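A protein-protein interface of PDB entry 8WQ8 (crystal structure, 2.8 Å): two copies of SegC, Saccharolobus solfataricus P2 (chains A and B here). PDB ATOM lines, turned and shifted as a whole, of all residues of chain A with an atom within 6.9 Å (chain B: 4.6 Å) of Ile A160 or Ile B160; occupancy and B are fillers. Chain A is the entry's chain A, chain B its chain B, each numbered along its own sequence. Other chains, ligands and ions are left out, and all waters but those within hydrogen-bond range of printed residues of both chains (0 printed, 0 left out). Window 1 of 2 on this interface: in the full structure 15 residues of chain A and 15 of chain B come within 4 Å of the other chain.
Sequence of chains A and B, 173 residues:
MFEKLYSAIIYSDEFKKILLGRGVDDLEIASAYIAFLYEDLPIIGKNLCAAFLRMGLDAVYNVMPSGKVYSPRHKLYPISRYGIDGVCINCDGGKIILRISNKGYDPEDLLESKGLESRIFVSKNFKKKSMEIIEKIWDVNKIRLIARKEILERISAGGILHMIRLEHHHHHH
Of the printed residues of chain B, Ile A160 touches Ile B18, Leu B19, Ile B160 and Met B163.
Printed residues of chain A within 4 Å of Ile B160: Ile A18, Leu A19, Ile A160 and Ile A164.
Of the printed residues of chain A, Leu B19 touches Gly A159, Ile A160 and Leu A161.
Of the printed residues of chain B, Ser A156 touches Ile B18 (3.4 Å).
Of the printed residues of chain A, Ile B18 touches Ser A156 (3.4 Å), Gly A159 (3.3 Å) and Ile A160 (2.8 Å).
His B162 touches none of the printed residues of chain A.
Met A163 touches none of the printed residues of chain B.
The nearest printed residue of chain B that does not touch Leu A19 is Gly B158 (4.8 Å).
Among the printed residues, merely in contact across the chains: Ile A18 with Ile B155, Ile A18 with Gly B159, Leu A19 with Gly B159, Leu A20 with Gly B158, Leu A20 with Gly B159, Leu A20 with Leu B161, Gly A21 with Gly B158, Gly A21 with Gly B159, Ser A156 with Ile B18, Gly A159 with Ile B18, Gly A159 with Leu B19, Ile A160 with Ile B160, Ile A160 with Met B163, Leu A161 with Ile B164, Ile A164 with Ile B160, Ile A164 with Leu B161 and Ile A164 with Ile B164.
N of Ile B160 lies within hydrogen-bond range of O of Ile A18 (2.8 Å).
The backbone NH (N) of Ile B160 is in hydrogen-bond range of the backbone carbonyl oxygen (O) of Leu A19.
O of Leu A19 is in hydrogen-bond range of N of Leu B161, 3.2 Å away.
O of Ile B18 is in hydrogen-bond range of N of Ile A160 (2.8 Å).
The backbone NH of Ile A160 is in hydrogen-bond range of the backbone carbonyl oxygen of Leu B19.
O of Leu B19 sits at hydrogen-bond distance from N of Leu A161, 3.4 Å away.
O of Lys A16 is in hydrogen-bond range of N of Gly A21.
Of the 18 printed residues of chain A, 9 touch a printed residue of chain B.
Hydrophobic or aromatic side chains of chain A that line the printed part of chain B: Ile A18, Leu A20, Ile A160, Leu A161 and Ile A164.
Of the 10 printed residues of chain B, 9 touch a printed residue of chain A.
Printed residues of chain B that touch a printed residue of chain A: Ile B18, Leu B19, Ile B155, Gly B158, Gly B159, Ile B160, Leu B161, Met B163 and Ile B164.
Hydrophobic or aromatic side chains of chain B that line the printed part of chain A: Ile B18, Leu B19, Ile B155, Ile B160, Leu B161, Met B163 and Ile B164.
Among the printed residues, 23 pairs touch across the chains.
Ile A18 touches Ile B155, but with the chains exchanged Ile A155 does not touch Ile B18 (4.2 Å).
Ile A18 touches Ile B160, and with the chains exchanged Ile A160 touches Ile B18.
Leu A19 touches Ile B160, and with the chains exchanged Ile A160 touches Leu B19.
Leu A19 touches Leu B161, and with the chains exchanged Leu A161 touches Leu B19.
Positions printed for both chains: 18, 19, 155, 158, 159, 160, 161, 162, 163 and 164.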
ATOM      1  N   PHE A  15       9.563  34.241  -1.727  1.00  0.00           N
ATOM      2  CA  PHE A  15      10.080  34.082  -0.372  1.00  0.00           C
ATOM      3  C   PHE A  15       8.972  34.221   0.667  1.00  0.00           C
ATOM      4  O   PHE A  15       8.969  33.501   1.680  1.00  0.00           O
ATOM      5  CB  PHE A  15      11.197  35.084  -0.089  1.00  0.00           C
ATOM      6  CG  PHE A  15      11.660  35.077   1.349  1.00  0.00           C
ATOM      7  CD1 PHE A  15      12.446  34.031   1.835  1.00  0.00           C
ATOM      8  CD2 PHE A  15      11.291  36.105   2.221  1.00  0.00           C
ATOM      9  CE1 PHE A  15      12.861  34.005   3.156  1.00  0.00           C
ATOM     10  CE2 PHE A  15      11.697  36.089   3.554  1.00  0.00           C
ATOM     11  CZ  PHE A  15      12.490  35.040   4.023  1.00  0.00           C
ATOM     12  N   LYS A  16       8.019  35.139   0.439  1.00  0.00           N
ATOM     13  CA  LYS A  16       6.931  35.287   1.406  1.00  0.00           C
ATOM     14  C   LYS A  16       6.035  34.047   1.437  1.00  0.00           C
ATOM     15  O   LYS A  16       5.558  33.655   2.512  1.00  0.00           O
ATOM     16  CB  LYS A  16       6.106  36.544   1.122  1.00  0.00           C
ATOM     17  CG  LYS A  16       5.263  37.004   2.317  1.00  0.00           C
ATOM     18  CD  LYS A  16       4.334  38.157   1.946  1.00  0.00           C
ATOM     19  CE  LYS A  16       3.391  38.495   3.087  1.00  0.00           C
ATOM     20  NZ  LYS A  16       2.315  39.452   2.686  1.00  0.00           N
ATOM     21  N   LYS A  17       5.793  33.409   0.281  1.00  0.00           N
ATOM     22  CA  LYS A  17       5.056  32.150   0.313  1.00  0.00           C
ATOM     23  C   LYS A  17       5.793  31.112   1.157  1.00  0.00           C
ATOM     24  O   LYS A  17       5.174  30.382   1.940  1.00  0.00           O
ATOM     25  CB  LYS A  17       4.826  31.628  -1.097  1.00  0.00           C
ATOM     26  CG  LYS A  17       3.925  32.495  -1.948  1.00  0.00           C
ATOM     27  CD  LYS A  17       3.753  31.813  -3.282  1.00  0.00           C
ATOM     28  CE  LYS A  17       3.306  32.727  -4.398  1.00  0.00           C
ATOM     29  NZ  LYS A  17       3.575  32.020  -5.692  1.00  0.00           N
ATOM     30  N   ILE A  18       7.123  31.049   1.038  1.00  0.00           N
ATOM     31  CA  ILE A  18       7.882  30.130   1.873  1.00  0.00           C
ATOM     32  C   ILE A  18       7.793  30.535   3.340  1.00  0.00           C
ATOM     33  O   ILE A  18       7.643  29.683   4.224  1.00  0.00           O
ATOM     34  CB  ILE A  18       9.334  30.054   1.377  1.00  0.00           C
ATOM     35  CG1 ILE A  18       9.356  29.317   0.041  1.00  0.00           C
ATOM     36  CG2 ILE A  18      10.245  29.377   2.429  1.00  0.00           C
ATOM     37  CD1 ILE A  18      10.486  29.700  -0.850  1.00  0.00           C
ATOM     38  N   LEU A  19       7.849  31.836   3.620  1.00  0.00           N
ATOM     39  CA  LEU A  19       8.009  32.272   5.001  1.00  0.00           C
ATOM     40  C   LEU A  19       6.681  32.340   5.743  1.00  0.00           C
ATOM     41  O   LEU A  19       6.594  31.895   6.893  1.00  0.00           O
ATOM     42  CB  LEU A  19       8.713  33.628   5.048  1.00  0.00           C
ATOM     43  CG  LEU A  19       9.015  34.158   6.448  1.00  0.00           C
ATOM     44  CD1 LEU A  19      10.314  33.573   6.993  1.00  0.00           C
ATOM     45  CD2 LEU A  19       9.058  35.673   6.414  1.00  0.00           C
ATOM     46  N   LEU A  20       5.641  32.895   5.112  1.00  0.00           N
ATOM     47  CA  LEU A  20       4.346  33.089   5.764  1.00  0.00           C
ATOM     48  C   LEU A  20       3.193  32.407   5.048  1.00  0.00           C
ATOM     49  O   LEU A  20       2.043  32.581   5.460  1.00  0.00           O
ATOM     50  CB  LEU A  20       4.015  34.582   5.917  1.00  0.00           C
ATOM     51  CG  LEU A  20       5.106  35.519   6.422  1.00  0.00           C
ATOM     52  CD1 LEU A  20       4.666  36.932   6.203  1.00  0.00           C
ATOM     53  CD2 LEU A  20       5.383  35.261   7.891  1.00  0.00           C
ATOM     54  N   GLY A  21       3.450  31.663   3.981  1.00  0.00           N
ATOM     55  CA  GLY A  21       2.387  30.910   3.349  1.00  0.00           C
ATOM     56  C   GLY A  21       1.451  31.709   2.473  1.00  0.00           C
ATOM     57  O   GLY A  21       0.458  31.150   1.996  1.00  0.00           O
ATOM     58  N   ILE A 155      18.300  29.627   2.124  1.00  0.00           N
ATOM     59  CA  ILE A 155      17.814  29.230   3.438  1.00  0.00           C
ATOM     60  C   ILE A 155      18.638  28.073   3.968  1.00  0.00           C
ATOM     61  O   ILE A 155      18.971  28.025   5.158  1.00  0.00           O
ATOM     62  CB  ILE A 155      16.314  28.887   3.378  1.00  0.00           C
ATOM     63  CG1 ILE A 155      15.511  30.090   2.858  1.00  0.00           C
ATOM     64  CG2 ILE A 155      15.823  28.428   4.753  1.00  0.00           C
ATOM     65  CD1 ILE A 155      14.034  29.802   2.609  1.00  0.00           C
ATOM     66  N   SER A 156      19.035  27.151   3.082  1.00  0.00           N
ATOM     67  CA  SER A 156      19.765  25.952   3.484  1.00  0.00           C
ATOM     68  C   SER A 156      21.246  26.200   3.739  1.00  0.00           C
ATOM     69  O   SER A 156      21.931  25.288   4.211  1.00  0.00           O
ATOM     70  CB  SER A 156      19.607  24.854   2.427  1.00  0.00           C
ATOM     71  OG  SER A 156      18.242  24.523   2.227  1.00  0.00           O
ATOM     72  N   ALA A 157      21.762  27.388   3.427  1.00  0.00           N
ATOM     73  CA  ALA A 157      23.134  27.725   3.788  1.00  0.00           C
ATOM     74  C   ALA A 157      23.382  27.454   5.267  1.00  0.00           C
ATOM     75  O   ALA A 157      24.189  26.594   5.636  1.00  0.00           O
ATOM     76  CB  ALA A 157      23.417  29.190   3.442  1.00  0.00           C
ATOM     77  N   GLY A 158      22.650  28.148   6.128  1.00  0.00           N
ATOM     78  CA  GLY A 158      22.798  27.947   7.552  1.00  0.00           C
ATOM     79  C   GLY A 158      21.533  27.452   8.212  1.00  0.00           C
ATOM     80  O   GLY A 158      21.533  27.174   9.412  1.00  0.00           O
ATOM     81  N   GLY A 159      20.451  27.345   7.452  1.00  0.00           N
ATOM     82  CA  GLY A 159      19.252  26.715   7.955  1.00  0.00           C
ATOM     83  C   GLY A 159      18.155  27.721   8.242  1.00  0.00           C
ATOM     84  O   GLY A 159      18.390  28.911   8.419  1.00  0.00           O
ATOM     85  N   ILE A 160      16.923  27.213   8.253  1.00  0.00           N
ATOM     86  CA  ILE A 160      15.759  28.017   8.610  1.00  0.00           C
ATOM     87  C   ILE A 160      16.036  28.750   9.909  1.00  0.00           C
ATOM     88  O   ILE A 160      15.917  29.976  10.000  1.00  0.00           O
ATOM     89  CB  ILE A 160      14.516  27.123   8.759  1.00  0.00           C
ATOM     90  CG1 ILE A 160      13.867  26.811   7.417  1.00  0.00           C
ATOM     91  CG2 ILE A 160      13.489  27.808   9.655  1.00  0.00           C
ATOM     92  CD1 ILE A 160      12.519  26.064   7.550  1.00  0.00           C
ATOM     93  N   LEU A 161      16.440  27.994  10.926  1.00  0.00           N
ATOM     94  CA  LEU A 161      16.421  28.514  12.282  1.00  0.00           C
ATOM     95  C   LEU A 161      17.485  29.581  12.474  1.00  0.00           C
ATOM     96  O   LEU A 161      17.233  30.614  13.106  1.00  0.00           O
ATOM     97  CB  LEU A 161      16.605  27.372  13.275  1.00  0.00           C
ATOM     98  CG  LEU A 161      15.489  26.328  13.196  1.00  0.00           C
ATOM     99  CD1 LEU A 161      15.917  25.016  13.871  1.00  0.00           C
ATOM    100  CD2 LEU A 161      14.152  26.848  13.708  1.00  0.00           C
ATOM    101  N   HIS A 162      18.685  29.351  11.941  1.00  0.00           N
ATOM    102  CA  HIS A 162      19.702  30.395  11.975  1.00  0.00           C
ATOM    103  C   HIS A 162      19.298  31.604  11.124  1.00  0.00           C
ATOM    104  O   HIS A 162      19.566  32.750  11.507  1.00  0.00           O
ATOM    105  CB  HIS A 162      21.046  29.790  11.546  1.00  0.00           C
ATOM    106  CG  HIS A 162      21.996  30.755  10.899  1.00  0.00           C
ATOM    107  ND1 HIS A 162      21.806  31.258   9.626  1.00  0.00           N
ATOM    108  CD2 HIS A 162      23.170  31.273  11.334  1.00  0.00           C
ATOM    109  CE1 HIS A 162      22.811  32.059   9.314  1.00  0.00           C
ATOM    110  NE2 HIS A 162      23.653  32.085  10.333  1.00  0.00           N
ATOM    111  N   MET A 163      18.629  31.380   9.991  1.00  0.00           N
ATOM    112  CA  MET A 163      18.289  32.494   9.113  1.00  0.00           C
ATOM    113  C   MET A 163      17.238  33.400   9.754  1.00  0.00           C
ATOM    114  O   MET A 163      17.346  34.631   9.687  1.00  0.00           O
ATOM    115  CB  MET A 163      17.798  31.961   7.768  1.00  0.00           C
ATOM    116  CG  MET A 163      17.082  32.996   6.935  1.00  0.00           C
ATOM    117  SD  MET A 163      15.538  32.415   6.195  1.00  0.00           S
ATOM    118  CE  MET A 163      14.365  32.656   7.540  1.00  0.00           C
ATOM    119  N   ILE A 164      16.204  32.804  10.360  1.00  0.00           N
ATOM    120  CA  ILE A 164      15.231  33.561  11.155  1.00  0.00           C
ATOM    121  C   ILE A 164      15.932  34.344  12.257  1.00  0.00           C
ATOM    122  O   ILE A 164      15.710  35.552  12.425  1.00  0.00           O
ATOM    123  CB  ILE A 164      14.187  32.612  11.766  1.00  0.00           C
ATOM    124  CG1 ILE A 164      13.099  32.269  10.762  1.00  0.00           C
ATOM    125  CG2 ILE A 164      13.587  33.224  13.045  1.00  0.00           C
ATOM    126  CD1 ILE A 164      12.136  31.271  11.327  1.00  0.00           C
ATOM    127  N   ARG A 165      16.749  33.646  13.055  1.00  0.00           N
ATOM    128  CA  ARG A 165      17.507  34.208  14.176  1.00  0.00           C
ATOM    129  C   ARG A 165      18.578  35.224  13.694  1.00  0.00           C
ATOM    130  O   ARG A 165      18.313  36.147  12.897  1.00  0.00           O
ATOM    131  CB  ARG A 165      18.141  33.044  14.992  1.00  0.00           C
ATOM    132  CG  ARG A 165      19.230  33.426  16.028  1.00  0.00           C
ATOM    133  CD  ARG A 165      20.692  33.502  15.435  1.00  0.00           C
ATOM    134  NE  ARG A 165      21.520  32.284  15.487  1.00  0.00           N
ATOM    135  CZ  ARG A 165      22.853  32.263  15.364  1.00  0.00           C
ATOM    136  NH1 ARG A 165      23.553  33.380  15.175  1.00  0.00           N
ATOM    137  NH2 ARG A 165      23.501  31.091  15.407  1.00  0.00           N
ATOM    138  N   ILE B  18      17.605  21.938   5.114  1.00  0.00           N
ATOM    139  CA  ILE B  18      16.785  23.143   5.136  1.00  0.00           C
ATOM    140  C   ILE B  18      16.677  23.685   6.556  1.00  0.00           C
ATOM    141  O   ILE B  18      16.744  24.898   6.770  1.00  0.00           O
ATOM    142  CB  ILE B  18      15.399  22.862   4.513  1.00  0.00           C
ATOM    143  CG1 ILE B  18      15.520  22.635   3.003  1.00  0.00           C
ATOM    144  CG2 ILE B  18      14.403  23.991   4.810  1.00  0.00           C
ATOM    145  CD1 ILE B  18      14.306  21.995   2.386  1.00  0.00           C
ATOM    146  N   LEU B  19      16.534  22.810   7.551  1.00  0.00           N
ATOM    147  CA  LEU B  19      16.209  23.293   8.889  1.00  0.00           C
ATOM    148  C   LEU B  19      17.441  23.786   9.648  1.00  0.00           C
ATOM    149  O   LEU B  19      17.375  24.812  10.332  1.00  0.00           O
ATOM    150  CB  LEU B  19      15.501  22.194   9.696  1.00  0.00           C
ATOM    151  CG  LEU B  19      14.906  22.647  11.047  1.00  0.00           C
ATOM    152  CD1 LEU B  19      13.818  23.686  10.838  1.00  0.00           C
ATOM    153  CD2 LEU B  19      14.377  21.497  11.871  1.00  0.00           C
ATOM    154  N   ILE B 155       6.260  22.932   3.500  1.00  0.00           N
ATOM    155  CA  ILE B 155       6.597  24.123   4.288  1.00  0.00           C
ATOM    156  C   ILE B 155       5.740  25.326   3.879  1.00  0.00           C
ATOM    157  O   ILE B 155       5.179  26.034   4.724  1.00  0.00           O
ATOM    158  CB  ILE B 155       8.090  24.447   4.136  1.00  0.00           C
ATOM    159  CG1 ILE B 155       8.944  23.384   4.815  1.00  0.00           C
ATOM    160  CG2 ILE B 155       8.373  25.817   4.684  1.00  0.00           C
ATOM    161  CD1 ILE B 155      10.432  23.596   4.606  1.00  0.00           C
ATOM    162  N   GLY B 158       1.560  26.541   5.211  1.00  0.00           N
ATOM    163  CA  GLY B 158       1.337  27.560   6.216  1.00  0.00           C
ATOM    164  C   GLY B 158       2.533  28.469   6.437  1.00  0.00           C
ATOM    165  O   GLY B 158       2.446  29.424   7.214  1.00  0.00           O
ATOM    166  N   GLY B 159       3.648  28.182   5.774  1.00  0.00           N
ATOM    167  CA  GLY B 159       4.872  28.960   5.876  1.00  0.00           C
ATOM    168  C   GLY B 159       5.798  28.450   6.961  1.00  0.00           C
ATOM    169  O   GLY B 159       5.378  27.857   7.953  1.00  0.00           O
ATOM    170  N   ILE B 160       7.094  28.687   6.750  1.00  0.00           N
ATOM    171  CA  ILE B 160       8.168  28.324   7.669  1.00  0.00           C
ATOM    172  C   ILE B 160       7.803  28.667   9.100  1.00  0.00           C
ATOM    173  O   ILE B 160       8.042  27.883  10.019  1.00  0.00           O
ATOM    174  CB  ILE B 160       9.461  29.054   7.283  1.00  0.00           C
ATOM    175  CG1 ILE B 160      10.125  28.381   6.087  1.00  0.00           C
ATOM    176  CG2 ILE B 160      10.396  29.149   8.486  1.00  0.00           C
ATOM    177  CD1 ILE B 160      11.564  28.812   5.870  1.00  0.00           C
ATOM    178  N   LEU B 161       7.221  29.849   9.291  1.00  0.00           N
ATOM    179  CA  LEU B 161       7.008  30.376  10.634  1.00  0.00           C
ATOM    180  C   LEU B 161       5.986  29.545  11.391  1.00  0.00           C
ATOM    181  O   LEU B 161       6.237  29.128  12.528  1.00  0.00           O
ATOM    182  CB  LEU B 161       6.556  31.835  10.556  1.00  0.00           C
ATOM    183  CG  LEU B 161       7.640  32.867  10.197  1.00  0.00           C
ATOM    184  CD1 LEU B 161       7.297  34.224  10.739  1.00  0.00           C
ATOM    185  CD2 LEU B 161       9.022  32.458  10.647  1.00  0.00           C
ATOM    186  N   HIS B 162       4.825  29.298  10.781  1.00  0.00           N
ATOM    187  CA  HIS B 162       3.820  28.465  11.436  1.00  0.00           C
ATOM    188  C   HIS B 162       4.336  27.047  11.700  1.00  0.00           C
ATOM    189  O   HIS B 162       3.975  26.430  12.711  1.00  0.00           O
ATOM    190  CB  HIS B 162       2.541  28.447  10.591  1.00  0.00           C
ATOM    191  CG  HIS B 162       1.723  27.204  10.756  1.00  0.00           C
ATOM    192  ND1 HIS B 162       1.646  26.229   9.779  1.00  0.00           N
ATOM    193  CD2 HIS B 162       0.962  26.764  11.787  1.00  0.00           C
ATOM    194  CE1 HIS B 162       0.866  25.247  10.199  1.00  0.00           C
ATOM    195  NE2 HIS B 162       0.439  25.546  11.415  1.00  0.00           N
ATOM    196  N   MET B 163       5.206  26.530  10.829  1.00  0.00           N
ATOM    197  CA  MET B 163       5.599  25.127  10.914  1.00  0.00           C
ATOM    198  C   MET B 163       6.498  24.878  12.125  1.00  0.00           C
ATOM    199  O   MET B 163       6.176  24.047  12.984  1.00  0.00           O
ATOM    200  CB  MET B 163       6.254  24.695   9.595  1.00  0.00           C
ATOM    201  CG  MET B 163       6.999  23.374   9.626  1.00  0.00           C
ATOM    202  SD  MET B 163       8.250  23.253   8.312  1.00  0.00           S
ATOM    203  CE  MET B 163       9.671  24.064   9.049  1.00  0.00           C
ATOM    204  N   ILE B 164       7.615  25.610  12.236  1.00  0.00           N
ATOM    205  CA  ILE B 164       8.469  25.424  13.412  1.00  0.00           C
ATOM    206  C   ILE B 164       7.776  25.937  14.670  1.00  0.00           C
ATOM    207  O   ILE B 164       8.062  25.460  15.779  1.00  0.00           O
ATOM    208  CB  ILE B 164       9.853  26.090  13.247  1.00  0.00           C
ATOM    209  CG1 ILE B 164       9.771  27.609  13.376  1.00  0.00           C
ATOM    210  CG2 ILE B 164      10.482  25.715  11.919  1.00  0.00           C
ATOM    211  CD1 ILE B 164      11.001  28.314  12.841  1.00  0.00           C
